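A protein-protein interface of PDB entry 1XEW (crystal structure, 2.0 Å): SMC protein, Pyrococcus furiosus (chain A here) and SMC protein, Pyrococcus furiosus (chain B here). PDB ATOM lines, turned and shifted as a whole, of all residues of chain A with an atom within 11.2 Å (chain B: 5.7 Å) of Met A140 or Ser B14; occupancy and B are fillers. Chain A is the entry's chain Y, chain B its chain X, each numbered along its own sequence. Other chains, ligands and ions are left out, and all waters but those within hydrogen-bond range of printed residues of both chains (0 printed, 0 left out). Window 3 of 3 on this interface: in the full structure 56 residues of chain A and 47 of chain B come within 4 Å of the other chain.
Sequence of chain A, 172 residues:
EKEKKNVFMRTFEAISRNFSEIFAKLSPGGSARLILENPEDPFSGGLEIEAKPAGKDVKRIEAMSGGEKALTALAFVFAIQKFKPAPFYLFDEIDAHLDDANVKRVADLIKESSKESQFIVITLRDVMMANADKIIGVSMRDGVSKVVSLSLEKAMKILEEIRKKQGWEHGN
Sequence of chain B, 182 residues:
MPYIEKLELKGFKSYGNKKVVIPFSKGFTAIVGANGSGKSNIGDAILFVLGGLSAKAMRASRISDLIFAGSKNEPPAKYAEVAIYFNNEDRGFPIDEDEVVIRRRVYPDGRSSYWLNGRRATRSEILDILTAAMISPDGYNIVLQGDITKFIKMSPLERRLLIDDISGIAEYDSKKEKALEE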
ATOM      1  N   GLY A 137      12.387  13.326  24.142  1.00  0.00           N
ATOM      2  CA  GLY A 137      11.504  14.284  24.842  1.00  0.00           C
ATOM      3  C   GLY A 137      10.888  15.201  23.841  1.00  0.00           C
ATOM      4  O   GLY A 137      11.530  15.531  22.837  1.00  0.00           O
ATOM      5  N   VAL A 138       9.659  15.631  24.061  1.00  0.00           N
ATOM      6  CA  VAL A 138       9.029  16.490  23.070  1.00  0.00           C
ATOM      7  C   VAL A 138       8.448  17.678  23.823  1.00  0.00           C
ATOM      8  O   VAL A 138       7.832  17.521  24.906  1.00  0.00           O
ATOM      9  CB  VAL A 138       7.762  15.785  22.370  1.00  0.00           C
ATOM     10  CG1 VAL A 138       7.199  16.648  21.171  1.00  0.00           C
ATOM     11  CG2 VAL A 138       8.098  14.428  21.919  1.00  0.00           C
ATOM     12  N   SER A 139       8.557  18.851  23.219  1.00  0.00           N
ATOM     13  CA  SER A 139       8.013  20.081  23.844  1.00  0.00           C
ATOM     14  C   SER A 139       7.637  21.088  22.751  1.00  0.00           C
ATOM     15  O   SER A 139       8.152  21.010  21.621  1.00  0.00           O
ATOM     16  CB  SER A 139       9.074  20.721  24.783  1.00  0.00           C
ATOM     17  OG  SER A 139      10.306  21.002  24.093  1.00  0.00           O
ATOM     18  N   MET A 140       6.746  22.011  23.085  1.00  0.00           N
ATOM     19  CA  MET A 140       6.296  23.037  22.161  1.00  0.00           C
ATOM     20  C   MET A 140       6.799  24.416  22.567  1.00  0.00           C
ATOM     21  O   MET A 140       6.954  24.696  23.782  1.00  0.00           O
ATOM     22  CB  MET A 140       4.773  23.080  22.101  1.00  0.00           C
ATOM     23  CG  MET A 140       4.191  24.170  21.118  1.00  0.00           C
ATOM     24  SD  MET A 140       2.568  23.757  20.785  1.00  0.00           S
ATOM     25  CE  MET A 140       2.923  22.153  19.837  1.00  0.00           C
ATOM     26  N   GLY A 143       1.903  26.860  17.322  1.00  0.00           N
ATOM     27  CA  GLY A 143       3.090  26.648  18.146  1.00  0.00           C
ATOM     28  C   GLY A 143       3.939  25.585  17.502  1.00  0.00           C
ATOM     29  O   GLY A 143       3.407  24.784  16.730  1.00  0.00           O
ATOM     30  N   VAL A 144       5.231  25.532  17.824  1.00  0.00           N
ATOM     31  CA  VAL A 144       6.082  24.532  17.219  1.00  0.00           C
ATOM     32  C   VAL A 144       6.656  23.461  18.186  1.00  0.00           C
ATOM     33  O   VAL A 144       7.169  23.781  19.273  1.00  0.00           O
ATOM     34  CB  VAL A 144       7.226  25.219  16.475  1.00  0.00           C
ATOM     35  CG1 VAL A 144       8.001  24.235  15.649  1.00  0.00           C
ATOM     36  CG2 VAL A 144       6.637  26.324  15.568  1.00  0.00           C
ATOM     37  N   SER A 145       6.534  22.203  17.777  1.00  0.00           N
ATOM     38  CA  SER A 145       7.077  21.067  18.551  1.00  0.00           C
ATOM     39  C   SER A 145       8.556  20.810  18.256  1.00  0.00           C
ATOM     40  O   SER A 145       9.015  20.964  17.131  1.00  0.00           O
ATOM     41  CB  SER A 145       6.279  19.808  18.273  1.00  0.00           C
ATOM     42  OG  SER A 145       4.936  19.984  18.564  1.00  0.00           O
ATOM     43  N   LYS A 146       9.289  20.358  19.264  1.00  0.00           N
ATOM     44  CA  LYS A 146      10.722  20.131  19.210  1.00  0.00           C
ATOM     45  C   LYS A 146      10.996  18.752  19.798  1.00  0.00           C
ATOM     46  O   LYS A 146      10.337  18.403  20.717  1.00  0.00           O
ATOM     47  CB  LYS A 146      11.366  21.199  20.121  1.00  0.00           C
ATOM     48  CG  LYS A 146      12.833  21.244  20.246  1.00  0.00           C
ATOM     49  CD  LYS A 146      13.250  22.072  21.510  1.00  0.00           C
ATOM     50  CE  LYS A 146      13.409  21.119  22.766  1.00  0.00           C
ATOM     51  NZ  LYS A 146      13.524  21.790  24.095  1.00  0.00           N
ATOM     52  N   VAL A 147      12.009  18.023  19.323  1.00  0.00           N
ATOM     53  CA  VAL A 147      12.272  16.713  19.823  1.00  0.00           C
ATOM     54  C   VAL A 147      13.774  16.624  20.115  1.00  0.00           C
ATOM     55  O   VAL A 147      14.556  17.282  19.428  1.00  0.00           O
ATOM     56  CB  VAL A 147      11.820  15.684  18.783  1.00  0.00           C
ATOM     57  CG1 VAL A 147      12.148  14.359  19.224  1.00  0.00           C
ATOM     58  CG2 VAL A 147      10.314  15.829  18.553  1.00  0.00           C
ATOM     59  N   VAL A 148      14.139  15.877  21.167  1.00  0.00           N
ATOM     60  CA  VAL A 148      15.527  15.714  21.660  1.00  0.00           C
ATOM     61  C   VAL A 148      15.742  14.343  22.279  1.00  0.00           C
ATOM     62  O   VAL A 148      14.828  13.845  22.901  1.00  0.00           O
ATOM     63  CB  VAL A 148      15.872  16.696  22.825  1.00  0.00           C
ATOM     64  CG1 VAL A 148      17.357  16.595  23.101  1.00  0.00           C
ATOM     65  CG2 VAL A 148      15.483  18.158  22.479  1.00  0.00           C
ATOM     66  N   ILE A 158      12.396  16.353  33.781  1.00  0.00           N
ATOM     67  CA  ILE A 158      11.326  16.869  32.924  1.00  0.00           C
ATOM     68  C   ILE A 158      10.042  16.229  33.352  1.00  0.00           C
ATOM     69  O   ILE A 158       9.038  16.866  33.430  1.00  0.00           O
ATOM     70  CB  ILE A 158      11.623  16.600  31.343  1.00  0.00           C
ATOM     71  CG1 ILE A 158      12.612  17.661  30.829  1.00  0.00           C
ATOM     72  CG2 ILE A 158      10.291  16.714  30.490  1.00  0.00           C
ATOM     73  CD1 ILE A 158      13.779  17.014  30.098  1.00  0.00           C
ATOM     74  N   GLU A 161       8.726  17.781  36.264  1.00  0.00           N
ATOM     75  CA  GLU A 161       8.154  19.153  35.915  1.00  0.00           C
ATOM     76  C   GLU A 161       6.728  19.043  35.339  1.00  0.00           C
ATOM     77  O   GLU A 161       5.781  19.777  35.665  1.00  0.00           O
ATOM     78  CB  GLU A 161       9.025  19.858  34.837  1.00  0.00           C
ATOM     79  CG  GLU A 161      10.475  20.117  35.215  1.00  0.00           C
ATOM     80  CD  GLU A 161      11.236  20.903  34.152  1.00  0.00           C
ATOM     81  OE1 GLU A 161      12.377  21.344  34.446  1.00  0.00           O
ATOM     82  OE2 GLU A 161      10.717  21.085  33.020  1.00  0.00           O
ATOM     83  N   ILE A 162       6.554  18.062  34.459  1.00  0.00           N
ATOM     84  CA  ILE A 162       5.223  17.883  33.888  1.00  0.00           C
ATOM     85  C   ILE A 162       4.164  17.452  34.898  1.00  0.00           C
ATOM     86  O   ILE A 162       3.034  17.960  34.921  1.00  0.00           O
ATOM     87  CB  ILE A 162       5.265  16.809  32.738  1.00  0.00           C
ATOM     88  CG1 ILE A 162       6.098  17.372  31.541  1.00  0.00           C
ATOM     89  CG2 ILE A 162       3.793  16.473  32.304  1.00  0.00           C
ATOM     90  CD1 ILE A 162       6.787  16.262  30.708  1.00  0.00           C
ATOM     91  N   GLN A 166       0.503  18.969  35.603  1.00  0.00           N
ATOM     92  CA  GLN A 166      -0.685  18.218  35.284  1.00  0.00           C
ATOM     93  C   GLN A 166      -1.205  17.184  36.238  1.00  0.00           C
ATOM     94  O   GLN A 166      -2.354  16.797  36.100  1.00  0.00           O
ATOM     95  CB  GLN A 166      -0.639  17.572  33.863  1.00  0.00           C
ATOM     96  CG  GLN A 166       0.637  17.505  33.104  1.00  0.00           C
ATOM     97  CD  GLN A 166       0.493  16.805  31.674  1.00  0.00           C
ATOM     98  OE1 GLN A 166       0.200  15.588  31.543  1.00  0.00           O
ATOM     99  NE2 GLN A 166       0.740  17.586  30.634  1.00  0.00           N
ATOM    100  N   PHE B  12       4.069  19.334   9.322  1.00  0.00           N
ATOM    101  CA  PHE B  12       2.979  18.464   9.723  1.00  0.00           C
ATOM    102  C   PHE B  12       2.396  18.827  11.105  1.00  0.00           C
ATOM    103  O   PHE B  12       3.024  18.550  12.134  1.00  0.00           O
ATOM    104  CB  PHE B  12       3.467  17.010   9.777  1.00  0.00           C
ATOM    105  CG  PHE B  12       2.360  16.021  10.101  1.00  0.00           C
ATOM    106  CD1 PHE B  12       2.191  15.511  11.398  1.00  0.00           C
ATOM    107  CD2 PHE B  12       1.498  15.605   9.131  1.00  0.00           C
ATOM    108  CE1 PHE B  12       1.173  14.604  11.699  1.00  0.00           C
ATOM    109  CE2 PHE B  12       0.458  14.676   9.426  1.00  0.00           C
ATOM    110  CZ  PHE B  12       0.305  14.181  10.726  1.00  0.00           C
ATOM    111  N   LYS B  13       1.167  19.325  11.120  1.00  0.00           N
ATOM    112  CA  LYS B  13       0.505  19.738  12.353  1.00  0.00           C
ATOM    113  C   LYS B  13       1.410  20.655  13.115  1.00  0.00           C
ATOM    114  O   LYS B  13       1.854  21.694  12.560  1.00  0.00           O
ATOM    115  CB  LYS B  13       0.114  18.525  13.182  1.00  0.00           C
ATOM    116  CG  LYS B  13      -0.977  17.730  12.472  1.00  0.00           C
ATOM    117  CD  LYS B  13      -1.409  16.517  13.231  1.00  0.00           C
ATOM    118  CE  LYS B  13      -2.863  16.633  13.738  1.00  0.00           C
ATOM    119  NZ  LYS B  13      -3.374  15.334  14.478  1.00  0.00           N
ATOM    120  N   SER B  14       1.778  20.248  14.352  1.00  0.00           N
ATOM    121  CA  SER B  14       2.585  21.091  15.221  1.00  0.00           C
ATOM    122  C   SER B  14       4.056  21.144  14.878  1.00  0.00           C
ATOM    123  O   SER B  14       4.847  21.910  15.479  1.00  0.00           O
ATOM    124  CB  SER B  14       2.405  20.674  16.722  1.00  0.00           C
ATOM    125  OG  SER B  14       2.723  19.297  16.951  1.00  0.00           O
ATOM    126  N   TYR B  15       4.442  20.326  13.918  1.00  0.00           N
ATOM    127  CA  TYR B  15       5.810  20.299  13.547  1.00  0.00           C
ATOM    128  C   TYR B  15       5.942  21.273  12.366  1.00  0.00           C
ATOM    129  O   TYR B  15       5.340  21.042  11.250  1.00  0.00           O
ATOM    130  CB  TYR B  15       6.172  18.843  13.176  1.00  0.00           C
ATOM    131  CG  TYR B  15       6.160  17.917  14.425  1.00  0.00           C
ATOM    132  CD1 TYR B  15       7.326  17.636  15.096  1.00  0.00           C
ATOM    133  CD2 TYR B  15       4.979  17.418  14.927  1.00  0.00           C
ATOM    134  CE1 TYR B  15       7.340  16.882  16.270  1.00  0.00           C
ATOM    135  CE2 TYR B  15       4.965  16.644  16.082  1.00  0.00           C
ATOM    136  CZ  TYR B  15       6.134  16.394  16.745  1.00  0.00           C
ATOM    137  OH  TYR B  15       6.104  15.684  17.903  1.00  0.00           O
ATOM    138  N   GLY B  16       6.772  22.300  12.579  1.00  0.00           N
ATOM    139  CA  GLY B  16       6.984  23.349  11.585  1.00  0.00           C
ATOM    140  C   GLY B  16       7.794  23.106  10.312  1.00  0.00           C
ATOM    141  O   GLY B  16       8.051  21.955   9.911  1.00  0.00           O
ATOM    142  N   GLY B  36      -0.178  18.395  24.949  1.00  0.00           N
ATOM    143  CA  GLY B  36      -0.091  19.585  24.085  1.00  0.00           C
ATOM    144  C   GLY B  36       1.313  19.818  23.612  1.00  0.00           C
ATOM    145  O   GLY B  36       1.575  20.750  22.906  1.00  0.00           O
ATOM    146  N   SER B  37       2.263  18.965  23.936  1.00  0.00           N
ATOM    147  CA  SER B  37       3.619  19.220  23.432  1.00  0.00           C
ATOM    148  C   SER B  37       3.752  18.849  21.905  1.00  0.00           C
ATOM    149  O   SER B  37       4.704  19.281  21.263  1.00  0.00           O
ATOM    150  CB  SER B  37       4.589  18.329  24.190  1.00  0.00           C
ATOM    151  OG  SER B  37       4.099  16.966  24.030  1.00  0.00           O
ATOM    152  N   GLY B  38       2.854  17.995  21.398  1.00  0.00           N
ATOM    153  CA  GLY B  38       2.940  17.485  20.024  1.00  0.00           C
ATOM    154  C   GLY B  38       3.325  15.999  20.011  1.00  0.00           C
ATOM    155  O   GLY B  38       3.499  15.363  18.957  1.00  0.00           O
ATOM    156  N   ASN B  41       0.826  13.980  18.158  1.00  0.00           N
ATOM    157  CA  ASN B  41       0.927  14.110  16.699  1.00  0.00           C
ATOM    158  C   ASN B  41       1.910  13.045  16.106  1.00  0.00           C
ATOM    159  O   ASN B  41       1.944  12.840  14.904  1.00  0.00           O
ATOM    160  CB  ASN B  41       1.442  15.489  16.367  1.00  0.00           C
ATOM    161  CG  ASN B  41       0.370  16.508  16.460  1.00  0.00           C
ATOM    162  OD1 ASN B  41       0.635  17.702  16.625  1.00  0.00           O
ATOM    163  ND2 ASN B  41      -0.851  16.047  16.331  1.00  0.00           N
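Of the printed residues of chain B, Val A138 touches Tyr B15 and Ser B37.
Of chain B, only Ser B14 (3.5 Å), Gly B36 (3.6 Å) and Ser B37 (3.7 Å) come within 4 Å of Met A140.
Printed residues of chain B within 4 Å of Ser A145: Ser B14 (2.8 Å), Tyr B15 (3.7 Å), Ser B37 (2.8 Å) and Gly B38 (3.5 Å).
Lys A146 touches none of the printed residues of chain B.
Printed residues of chain B within 4 Å of Val A147: Tyr B15 (3.9 Å).
Glu A161 touches none of the printed residues of chain B.
No residue of chain A comes within 4 Å of Lys B13.
Ser B14 touches just these residues of chain A: Met A140 (3.5 Å), Gly A143 (3.4 Å), Val A144 (3.4 Å) and Ser A145 (2.8 Å).
Gly B16 touches one residue of chain A.
Of chain A, only Val A138 (3.4 Å), Ser A139 (3.8 Å), Met A140 (3.7 Å) and Ser A145 (2.8 Å) come within 4 Å of Ser B37.
Of chain A, only Ser A145 (3.5 Å) comes within 4 Å of Gly B38.
The nearest residue of chain B that does not touch Met A140 is Gly B38 (4.4 Å).
The side-chain hydroxyl (OG) of Ser B14 is in hydrogen-bond range of the side-chain amide oxygen (OD1) of Asn B41, 2.6 Å away.
O of Gly B38 lies within hydrogen-bond range of OH of Tyr B15, 2.8 Å away.
O of Ser A139 sits at hydrogen-bond distance from N of Lys A146, at 2.7 Å.
Hydrophobic or aromatic side chains of chain B that line the printed part of chain A: Tyr B15.
Among the printed residues, 14 pairs touch across the chains.
The side-chain hydroxyl of Ser B14 sits at hydrogen-bond distance from the side-chain hydroxyl of Ser A145, 2.8 Å away.
OG of Ser A145 is in hydrogen-bond range of O of Ser B37 (2.8 Å).
The backbone carbonyl oxygen (O) of Ser B14 lies close to the backbone carbonyl oxygen (O) of Gly A143, 3.4 Å away.
Val A138 touches Ser B37 (O to CB, 3.4 Å).
C of Ser A139 touches O of Ser B37 (3.8 Å).
Met A140 touches Ser B14.
Met A140 touches Gly B36.
Ser B37 touches Met A140 (O to CE, 3.7 Å).
Ser B14 touches Val A144.
Val A144 touches Gly B16.
Ser A145 touches Tyr B15 (CB to CE1, 3.7 Å).
Ser A145 touches Gly B38.
CG2 of Val A147 touches CE1 of Tyr B15, 3.9 Å away.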
